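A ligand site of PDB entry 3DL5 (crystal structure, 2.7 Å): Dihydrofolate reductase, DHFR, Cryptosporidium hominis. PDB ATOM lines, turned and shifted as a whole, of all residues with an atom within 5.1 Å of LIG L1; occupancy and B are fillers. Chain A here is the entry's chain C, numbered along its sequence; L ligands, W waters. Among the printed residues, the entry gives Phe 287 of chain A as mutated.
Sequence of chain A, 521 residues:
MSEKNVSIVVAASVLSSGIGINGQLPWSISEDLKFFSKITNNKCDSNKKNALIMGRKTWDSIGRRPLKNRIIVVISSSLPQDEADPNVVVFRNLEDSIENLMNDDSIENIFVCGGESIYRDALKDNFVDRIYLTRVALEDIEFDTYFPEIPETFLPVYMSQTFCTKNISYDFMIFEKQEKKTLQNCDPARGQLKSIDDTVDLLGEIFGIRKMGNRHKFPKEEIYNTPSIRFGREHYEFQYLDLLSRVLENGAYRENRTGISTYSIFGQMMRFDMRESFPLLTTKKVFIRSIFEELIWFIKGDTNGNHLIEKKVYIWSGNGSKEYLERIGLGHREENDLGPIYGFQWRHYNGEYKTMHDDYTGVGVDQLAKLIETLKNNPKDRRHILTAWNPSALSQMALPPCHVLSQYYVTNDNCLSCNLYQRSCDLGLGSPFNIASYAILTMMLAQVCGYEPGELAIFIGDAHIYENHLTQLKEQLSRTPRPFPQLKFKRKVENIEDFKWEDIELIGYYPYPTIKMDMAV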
ATOM      1  N   THR A 258      13.347  11.664 -24.359  1.00  0.00           N
ATOM      2  CA  THR A 258      12.425  12.572 -25.032  1.00  0.00           C
ATOM      3  C   THR A 258      12.617  14.045 -24.690  1.00  0.00           C
ATOM      4  O   THR A 258      12.186  14.901 -25.450  1.00  0.00           O
ATOM      5  CB  THR A 258      10.946  12.235 -24.710  1.00  0.00           C
ATOM      6  OG1 THR A 258      10.610  12.749 -23.410  1.00  0.00           O
ATOM      7  CG2 THR A 258      10.719  10.734 -24.744  1.00  0.00           C
ATOM      8  N   LYS A 284     -12.306   8.637 -19.103  1.00  0.00           N
ATOM      9  CA  LYS A 284     -11.915   9.468 -20.244  1.00  0.00           C
ATOM     10  C   LYS A 284     -12.258   8.665 -21.486  1.00  0.00           C
ATOM     11  O   LYS A 284     -12.304   7.437 -21.438  1.00  0.00           O
ATOM     12  CB  LYS A 284     -10.407   9.810 -20.217  1.00  0.00           C
ATOM     13  CG  LYS A 284      -9.500   8.848 -20.991  1.00  0.00           C
ATOM     14  CD  LYS A 284      -8.092   9.405 -21.143  1.00  0.00           C
ATOM     15  CE  LYS A 284      -7.196   8.430 -21.884  1.00  0.00           C
ATOM     16  NZ  LYS A 284      -5.827   8.959 -22.148  1.00  0.00           N
ATOM     17  N   PHE A 287      -9.931   5.782 -27.527  1.00  0.00           N
ATOM     18  CA  PHE A 287     -10.236   5.689 -28.953  1.00  0.00           C
ATOM     19  C   PHE A 287      -9.929   4.293 -29.481  1.00  0.00           C
ATOM     20  O   PHE A 287      -8.803   4.004 -29.901  1.00  0.00           O
ATOM     21  CB  PHE A 287      -9.451   6.737 -29.737  1.00  0.00           C
ATOM     22  CG  PHE A 287      -9.626   8.139 -29.226  1.00  0.00           C
ATOM     23  CD1 PHE A 287      -8.582   8.808 -28.605  1.00  0.00           C
ATOM     24  CD2 PHE A 287     -10.842   8.782 -29.354  1.00  0.00           C
ATOM     25  CE1 PHE A 287      -8.741  10.087 -28.130  1.00  0.00           C
ATOM     26  CE2 PHE A 287     -11.013  10.072 -28.879  1.00  0.00           C
ATOM     27  CZ  PHE A 287      -9.959  10.728 -28.272  1.00  0.00           C
ATOM     28  N   SER A 290      -8.362   2.771 -32.815  1.00  0.00           N
ATOM     29  CA  SER A 290      -6.927   2.845 -33.050  1.00  0.00           C
ATOM     30  C   SER A 290      -6.205   1.673 -32.392  1.00  0.00           C
ATOM     31  O   SER A 290      -5.134   1.259 -32.850  1.00  0.00           O
ATOM     32  CB  SER A 290      -6.371   4.175 -32.542  1.00  0.00           C
ATOM     33  OG  SER A 290      -7.173   5.258 -32.964  1.00  0.00           O
ATOM     34  N   GLU A 294      -4.188  -1.143 -34.591  1.00  0.00           N
ATOM     35  CA  GLU A 294      -2.763  -1.347 -34.379  1.00  0.00           C
ATOM     36  C   GLU A 294      -2.564  -2.833 -34.042  1.00  0.00           C
ATOM     37  O   GLU A 294      -1.514  -3.414 -34.307  1.00  0.00           O
ATOM     38  CB  GLU A 294      -2.276  -0.470 -33.224  1.00  0.00           C
ATOM     39  CG  GLU A 294      -0.854  -0.766 -32.768  1.00  0.00           C
ATOM     40  CD  GLU A 294      -0.545  -0.183 -31.396  1.00  0.00           C
ATOM     41  OE1 GLU A 294      -1.334  -0.423 -30.455  1.00  0.00           O
ATOM     42  OE2 GLU A 294       0.492   0.504 -31.247  1.00  0.00           O
ATOM     43  N   ILE A 315      -1.016   7.019 -34.296  1.00  0.00           N
ATOM     44  CA  ILE A 315      -0.206   6.776 -33.115  1.00  0.00           C
ATOM     45  C   ILE A 315       1.268   6.444 -33.351  1.00  0.00           C
ATOM     46  O   ILE A 315       2.077   6.518 -32.425  1.00  0.00           O
ATOM     47  CB  ILE A 315      -0.813   5.669 -32.231  1.00  0.00           C
ATOM     48  CG1 ILE A 315      -0.812   4.329 -32.974  1.00  0.00           C
ATOM     49  CG2 ILE A 315      -2.221   6.070 -31.806  1.00  0.00           C
ATOM     50  CD1 ILE A 315      -1.417   3.177 -32.178  1.00  0.00           C
ATOM     51  N   TRP A 316       1.645   6.064 -34.575  1.00  0.00           N
ATOM     52  CA  TRP A 316       3.047   5.765 -34.825  1.00  0.00           C
ATOM     53  C   TRP A 316       3.768   6.766 -35.714  1.00  0.00           C
ATOM     54  O   TRP A 316       4.925   6.566 -36.051  1.00  0.00           O
ATOM     55  CB  TRP A 316       3.220   4.356 -35.407  1.00  0.00           C
ATOM     56  CG  TRP A 316       3.128   3.267 -34.378  1.00  0.00           C
ATOM     57  CD1 TRP A 316       2.012   2.571 -34.004  1.00  0.00           C
ATOM     58  CD2 TRP A 316       4.196   2.785 -33.543  1.00  0.00           C
ATOM     59  NE1 TRP A 316       2.322   1.677 -33.008  1.00  0.00           N
ATOM     60  CE2 TRP A 316       3.652   1.789 -32.700  1.00  0.00           C
ATOM     61  CE3 TRP A 316       5.560   3.096 -33.436  1.00  0.00           C
ATOM     62  CZ2 TRP A 316       4.421   1.092 -31.754  1.00  0.00           C
ATOM     63  CZ3 TRP A 316       6.338   2.409 -32.485  1.00  0.00           C
ATOM     64  CH2 TRP A 316       5.757   1.425 -31.659  1.00  0.00           C
ATOM     65  N   ASN A 319       7.119   8.407 -34.099  1.00  0.00           N
ATOM     66  CA  ASN A 319       8.320   7.585 -34.117  1.00  0.00           C
ATOM     67  C   ASN A 319       8.574   6.996 -35.486  1.00  0.00           C
ATOM     68  O   ASN A 319       9.257   5.983 -35.626  1.00  0.00           O
ATOM     69  CB  ASN A 319       8.215   6.514 -33.030  1.00  0.00           C
ATOM     70  CG  ASN A 319       8.077   7.117 -31.640  1.00  0.00           C
ATOM     71  OD1 ASN A 319       6.962   7.321 -31.145  1.00  0.00           O
ATOM     72  ND2 ASN A 319       9.204   7.419 -31.018  1.00  0.00           N
ATOM     73  N   LEU A 399      11.734   1.984 -32.097  1.00  0.00           N
ATOM     74  CA  LEU A 399      11.622   2.053 -30.644  1.00  0.00           C
ATOM     75  C   LEU A 399      11.723   0.621 -30.123  1.00  0.00           C
ATOM     76  O   LEU A 399      11.141  -0.285 -30.700  1.00  0.00           O
ATOM     77  CB  LEU A 399      10.259   2.633 -30.281  1.00  0.00           C
ATOM     78  CG  LEU A 399      10.116   3.666 -29.160  1.00  0.00           C
ATOM     79  CD1 LEU A 399      11.185   4.748 -29.281  1.00  0.00           C
ATOM     80  CD2 LEU A 399       8.720   4.267 -29.243  1.00  0.00           C
ATOM     81  N   ASP A 426       3.794   4.603 -20.244  1.00  0.00           N
ATOM     82  CA  ASP A 426       3.328   5.978 -20.164  1.00  0.00           C
ATOM     83  C   ASP A 426       1.894   5.866 -19.656  1.00  0.00           C
ATOM     84  O   ASP A 426       0.981   5.588 -20.427  1.00  0.00           O
ATOM     85  CB  ASP A 426       3.377   6.599 -21.556  1.00  0.00           C
ATOM     86  CG  ASP A 426       2.731   7.958 -21.608  1.00  0.00           C
ATOM     87  OD1 ASP A 426       2.851   8.613 -22.669  1.00  0.00           O
ATOM     88  OD2 ASP A 426       2.091   8.374 -20.618  1.00  0.00           O
ATOM     89  N   LEU A 429      -0.905   8.154 -21.754  1.00  0.00           N
ATOM     90  CA  LEU A 429      -1.194   7.806 -23.148  1.00  0.00           C
ATOM     91  C   LEU A 429      -1.101   6.324 -23.480  1.00  0.00           C
ATOM     92  O   LEU A 429      -1.992   5.767 -24.108  1.00  0.00           O
ATOM     93  CB  LEU A 429      -0.298   8.640 -24.059  1.00  0.00           C
ATOM     94  CG  LEU A 429      -0.889   9.783 -24.866  1.00  0.00           C
ATOM     95  CD1 LEU A 429      -2.225  10.221 -24.307  1.00  0.00           C
ATOM     96  CD2 LEU A 429       0.108  10.925 -24.875  1.00  0.00           C
ATOM     97  N   GLY A 430      -0.171   5.608 -22.937  1.00  0.00           N
ATOM     98  CA  GLY A 430       0.183   4.304 -23.449  1.00  0.00           C
ATOM     99  C   GLY A 430      -0.692   3.292 -22.763  1.00  0.00           C
ATOM    100  O   GLY A 430      -1.399   2.519 -23.415  1.00  0.00           O
ATOM    101  N   SER A 431      -0.649   3.288 -21.437  1.00  0.00           N
ATOM    102  CA  SER A 431      -1.387   2.332 -20.638  1.00  0.00           C
ATOM    103  C   SER A 431      -2.834   2.056 -21.018  1.00  0.00           C
ATOM    104  O   SER A 431      -3.213   0.899 -21.204  1.00  0.00           O
ATOM    105  CB  SER A 431      -1.280   2.728 -19.168  1.00  0.00           C
ATOM    106  OG  SER A 431      -1.449   1.585 -18.364  1.00  0.00           O
ATOM    107  N   PHE A 433      -4.291   2.328 -23.762  1.00  0.00           N
ATOM    108  CA  PHE A 433      -4.207   1.568 -25.005  1.00  0.00           C
ATOM    109  C   PHE A 433      -3.743   0.139 -24.744  1.00  0.00           C
ATOM    110  O   PHE A 433      -4.322  -0.818 -25.256  1.00  0.00           O
ATOM    111  CB  PHE A 433      -3.212   2.231 -25.954  1.00  0.00           C
ATOM    112  CG  PHE A 433      -3.838   3.135 -26.962  1.00  0.00           C
ATOM    113  CD1 PHE A 433      -4.614   4.212 -26.553  1.00  0.00           C
ATOM    114  CD2 PHE A 433      -3.633   2.914 -28.315  1.00  0.00           C
ATOM    115  CE1 PHE A 433      -5.186   5.069 -27.498  1.00  0.00           C
ATOM    116  CE2 PHE A 433      -4.195   3.765 -29.268  1.00  0.00           C
ATOM    117  CZ  PHE A 433      -4.972   4.850 -28.854  1.00  0.00           C
ATOM    118  N   ASN A 434      -2.678  -0.006 -23.949  1.00  0.00           N
ATOM    119  CA  ASN A 434      -2.146  -1.337 -23.663  1.00  0.00           C
ATOM    120  C   ASN A 434      -3.135  -2.275 -23.010  1.00  0.00           C
ATOM    121  O   ASN A 434      -3.164  -3.474 -23.303  1.00  0.00           O
ATOM    122  CB  ASN A 434      -0.901  -1.251 -22.779  1.00  0.00           C
ATOM    123  CG  ASN A 434       0.277  -0.692 -23.492  1.00  0.00           C
ATOM    124  OD1 ASN A 434       0.762   0.393 -23.162  1.00  0.00           O
ATOM    125  ND2 ASN A 434       0.768  -1.419 -24.499  1.00  0.00           N
ATOM    126  N   TYR A 466       4.367  11.675 -17.701  1.00  0.00           N
ATOM    127  CA  TYR A 466       5.087  12.810 -18.261  1.00  0.00           C
ATOM    128  C   TYR A 466       4.534  14.130 -17.744  1.00  0.00           C
ATOM    129  O   TYR A 466       3.335  14.266 -17.523  1.00  0.00           O
ATOM    130  CB  TYR A 466       5.020  12.782 -19.789  1.00  0.00           C
ATOM    131  CG  TYR A 466       5.885  11.708 -20.423  1.00  0.00           C
ATOM    132  CD1 TYR A 466       7.158  11.994 -20.884  1.00  0.00           C
ATOM    133  CD2 TYR A 466       5.423  10.401 -20.552  1.00  0.00           C
ATOM    134  CE1 TYR A 466       7.944  11.011 -21.459  1.00  0.00           C
ATOM    135  CE2 TYR A 466       6.199   9.416 -21.125  1.00  0.00           C
ATOM    136  CZ  TYR A 466       7.459   9.729 -21.573  1.00  0.00           C
ATOM    137  OH  TYR A 466       8.243   8.752 -22.156  1.00  0.00           O
ATOM    138  N   ILE A 515      -9.653  13.621 -23.132  1.00  0.00           N
ATOM    139  CA  ILE A 515      -8.725  14.556 -22.512  1.00  0.00           C
ATOM    140  C   ILE A 515      -7.460  14.605 -23.351  1.00  0.00           C
ATOM    141  O   ILE A 515      -6.730  13.631 -23.425  1.00  0.00           O
ATOM    142  CB  ILE A 515      -8.364  14.117 -21.073  1.00  0.00           C
ATOM    143  CG1 ILE A 515      -9.608  14.112 -20.193  1.00  0.00           C
ATOM    144  CG2 ILE A 515      -7.307  15.047 -20.490  1.00  0.00           C
ATOM    145  CD1 ILE A 515      -9.393  13.554 -18.821  1.00  0.00           C
ATOM    146  N   MET A 517      -3.831  14.921 -24.623  1.00  0.00           N
ATOM    147  CA  MET A 517      -2.511  14.687 -24.041  1.00  0.00           C
ATOM    148  C   MET A 517      -1.472  14.466 -25.129  1.00  0.00           C
ATOM    149  O   MET A 517      -1.538  13.495 -25.889  1.00  0.00           O
ATOM    150  CB  MET A 517      -2.546  13.486 -23.094  1.00  0.00           C
ATOM    151  CG  MET A 517      -3.289  13.743 -21.795  1.00  0.00           C
ATOM    152  SD  MET A 517      -3.080  12.409 -20.603  1.00  0.00           S
ATOM    153  CE  MET A 517      -4.684  11.637 -20.655  1.00  0.00           C
ATOM    154  N   MET A 519       1.825  13.327 -26.902  1.00  0.00           N
ATOM    155  CA  MET A 519       2.839  12.290 -26.771  1.00  0.00           C
ATOM    156  C   MET A 519       4.245  12.870 -26.904  1.00  0.00           C
ATOM    157  O   MET A 519       4.463  13.842 -27.635  1.00  0.00           O
ATOM    158  CB  MET A 519       2.621  11.206 -27.829  1.00  0.00           C
ATOM    159  CG  MET A 519       3.296   9.874 -27.503  1.00  0.00           C
ATOM    160  SD  MET A 519       3.668   8.907 -28.971  1.00  0.00           S
ATOM    161  CE  MET A 519       4.738  10.036 -29.860  1.00  0.00           C
ATOM    162  N   ALA A 520       5.196  12.261 -26.205  1.00  0.00           N
ATOM    163  CA  ALA A 520       6.585  12.684 -26.270  1.00  0.00           C
ATOM    164  C   ALA A 520       7.384  11.811 -27.239  1.00  0.00           C
ATOM    165  O   ALA A 520       7.577  10.626 -26.993  1.00  0.00           O
ATOM    166  CB  ALA A 520       7.224  12.672 -24.888  1.00  0.00           C
HETATM  167  N1  LIG L   1       5.844   7.119 -26.535  1.00  0.00           N
HETATM  168  C1  LIG L   1       5.550   7.590 -25.323  1.00  0.00           C
HETATM  169  N2  LIG L   1       6.419   8.429 -24.731  1.00  0.00           N
HETATM  170  N3  LIG L   1       4.403   7.254 -24.698  1.00  0.00           N
HETATM  171  C2  LIG L   1       3.541   6.423 -25.300  1.00  0.00           C
HETATM  172  O1  LIG L   1       2.385   6.077 -24.678  1.00  0.00           O
HETATM  173  C3  LIG L   1       3.821   5.930 -26.549  1.00  0.00           C
HETATM  174  C4  LIG L   1       2.939   5.070 -27.180  1.00  0.00           C
HETATM  175  C5  LIG L   1       3.257   4.593 -28.431  1.00  0.00           C
HETATM  176  C6  LIG L   1       4.432   4.950 -29.051  1.00  0.00           C
HETATM  177  C7  LIG L   1       5.305   5.809 -28.418  1.00  0.00           C
HETATM  178  C8  LIG L   1       4.999   6.282 -27.161  1.00  0.00           C
HETATM  179  C9  LIG L   1       2.318   3.668 -29.145  1.00  0.00           C
HETATM  180  N4  LIG L   1       0.975   3.814 -28.652  1.00  0.00           N
HETATM  181  C10 LIG L   1      -1.023   7.443 -28.266  1.00  0.00           C
HETATM  182  C11 LIG L   1      -1.528   6.299 -27.684  1.00  0.00           C
HETATM  183  C12 LIG L   1      -0.840   5.113 -27.816  1.00  0.00           C
HETATM  184  C13 LIG L   1       0.338   5.047 -28.529  1.00  0.00           C
HETATM  185  C14 LIG L   1       0.829   6.186 -29.136  1.00  0.00           C
HETATM  186  C15 LIG L   1       0.147   7.387 -29.008  1.00  0.00           C
HETATM  187  C16 LIG L   1      -1.811   8.700 -28.148  1.00  0.00           C
HETATM  188  O2  LIG L   1      -1.303   9.798 -28.252  1.00  0.00           O
HETATM  189  N5  LIG L   1      -3.101   8.513 -27.974  1.00  0.00           N
HETATM  190  C17 LIG L   1      -4.092   9.563 -27.879  1.00  0.00           C
HETATM  191  C18 LIG L   1      -5.052   9.073 -28.932  1.00  0.00           C
HETATM  192  C19 LIG L   1      -5.210  10.036 -30.088  1.00  0.00           C
HETATM  193  C20 LIG L   1      -6.228   9.408 -31.002  1.00  0.00           C
HETATM  194  O3  LIG L   1      -6.369   8.173 -30.966  1.00  0.00           O
HETATM  195  O4  LIG L   1      -6.894  10.154 -31.749  1.00  0.00           O
HETATM  196  C21 LIG L   1      -4.839   9.512 -26.595  1.00  0.00           C
HETATM  197  O5  LIG L   1      -5.422  10.544 -26.200  1.00  0.00           O
HETATM  198  O6  LIG L   1      -4.859   8.444 -25.958  1.00  0.00           O
HETATM  199  C22 LIG L   1       0.224   2.633 -28.341  1.00  0.00           C
HETATM  200  C23 LIG L   1       0.368   2.318 -26.925  1.00  0.00           C
HETATM  201  C24 LIG L   1       0.488   2.037 -25.697  1.00  0.00           C
HETATM  202  N1  LG2 L   2       5.117   3.286 -24.267  1.00  0.00           N
HETATM  203  C1  LG2 L   2       4.045   2.632 -23.639  1.00  0.00           C
HETATM  204  N2  LG2 L   2       3.521   1.458 -24.196  1.00  0.00           N
HETATM  205  C2  LG2 L   2       3.877   1.058 -25.493  1.00  0.00           C
HETATM  206  C3  LG2 L   2       4.797   1.932 -26.342  1.00  0.00           C
HETATM  207  C4  LG2 L   2       5.777   2.715 -25.464  1.00  0.00           C
HETATM  208  O1  LG2 L   2       3.674   3.017 -22.533  1.00  0.00           O
HETATM  209  O2  LG2 L   2       3.446  -0.006 -25.944  1.00  0.00           O
HETATM  210  C5  LG2 L   2       5.756   4.452 -23.614  1.00  0.00           C
HETATM  211  C6  LG2 L   2       6.748   4.028 -22.534  1.00  0.00           C
HETATM  212  C7  LG2 L   2       7.599   5.299 -22.470  1.00  0.00           C
HETATM  213  C8  LG2 L   2       7.814   5.494 -23.977  1.00  0.00           C
HETATM  214  O3  LG2 L   2       6.845   6.393 -21.937  1.00  0.00           O
HETATM  215  O4  LG2 L   2       6.563   5.135 -24.597  1.00  0.00           O
HETATM  216  C9  LG2 L   2       8.920   4.543 -24.432  1.00  0.00           C
HETATM  217  O5  LG2 L   2      10.178   5.146 -24.150  1.00  0.00           O
HETATM  218  P1  LG2 L   2      11.436   4.315 -23.591  1.00  0.00           P
HETATM  219  O6  LG2 L   2      11.936   3.271 -24.506  1.00  0.00           O
HETATM  220  O7  LG2 L   2      12.548   5.436 -23.261  1.00  0.00           O
HETATM  221  O8  LG2 L   2      10.996   3.705 -22.168  1.00  0.00           O
HETATM  222  O   HOH W   1      -4.533   7.144 -23.952  1.00  0.00           O
HETATM  223  O   HOH W   2      -0.702  -0.581 -27.668  1.00  0.00           O
HETATM  224  O   HOH W   3      -6.491  10.788 -24.016  1.00  0.00           O
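The backbone NH (N) of Asp 426 lies within hydrogen-bond range of an oxygen (O1) of LG2 L2. OD1 of Asp 426 sits at hydrogen-bond distance from N3 of LIG L1, 2.9 Å away. N2 of LG2 L2 is in hydrogen-bond range of OD1 of Asn 434. An oxygen (O3) of LG2 L2 is in hydrogen-bond range of the side-chain hydroxyl (OH) of Tyr 466 (2.8 Å). O1 of LIG L1 sits close to N of Gly 430 (3.1 Å). NZ of Lys 284 lies within salt-bridge range of O6 of LIG L1, at 3.96 Å. The side-chain sulfur (SD) of Met 519 sits close to a nitrogen (N1) of LIG L1 (3.7 Å). N2 of LIG L1 is in hydrogen-bond range of OH of Tyr 466. A nitrogen (N2) of LIG L1 lies within hydrogen-bond range of the backbone carbonyl oxygen (O) of Ala 520 (3.4 Å).
A nitrogen (N1) of LIG L1 sits close to an oxygen (O4) of LG2 L2, at 2.9 Å.
The side-chain amide oxygen (OD1) of Asn 434 sits close to the backbone carbonyl oxygen (O) of Gly 430 (3.0 Å). The backbone NH (N) of Leu 429 is in hydrogen-bond range of the side-chain carboxylate (OD2) of Asp 426, 3.2 Å away. The side-chain carboxylate (OE2) of Glu 294 is in hydrogen-bond range of the indole nitrogen (NE1) of Trp 316, at 2.8 Å. O of Asp 426 sits at hydrogen-bond distance from N of Ser 431, 3.0 Å away.
CD1 of Phe 287 touches O3 of LIG L1, at 3.3 Å. Ser 290 touches LIG L1. OE2 of Glu 294 touches C22 of LIG L1, 3.6 Å away. Ile 315 touches LIG L1 (O to C14, 3.5 Å). Asn 319 touches LIG L1. Leu 399 touches LIG L1. Leu 429 touches LIG L1. Phe 433 touches LIG L1 (CD2 to C12, 3.6 Å). OD1 of Asn 434 touches C24 of LIG L1, at 3.0 Å. Hydrophobic or aromatic side chains that line LIG L1: Phe 287, Ile 315, Leu 399, Leu 429, Phe 433, Tyr 466 and Met 519. The nearest printed residue that does not touch LIG L1 is Trp 316 (4.2 Å).
Water W1 lies within hydrogen-bond range of O6 of LIG L1 (2.4 Å), NZ of Lys 284 (2.9 Å) and O of Leu 429 (2.9 Å). Water W3 lies within hydrogen-bond range of an oxygen (O5) of LIG L1, the side-chain amino group of Lys 284 and the backbone carbonyl oxygen of Ile 515.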
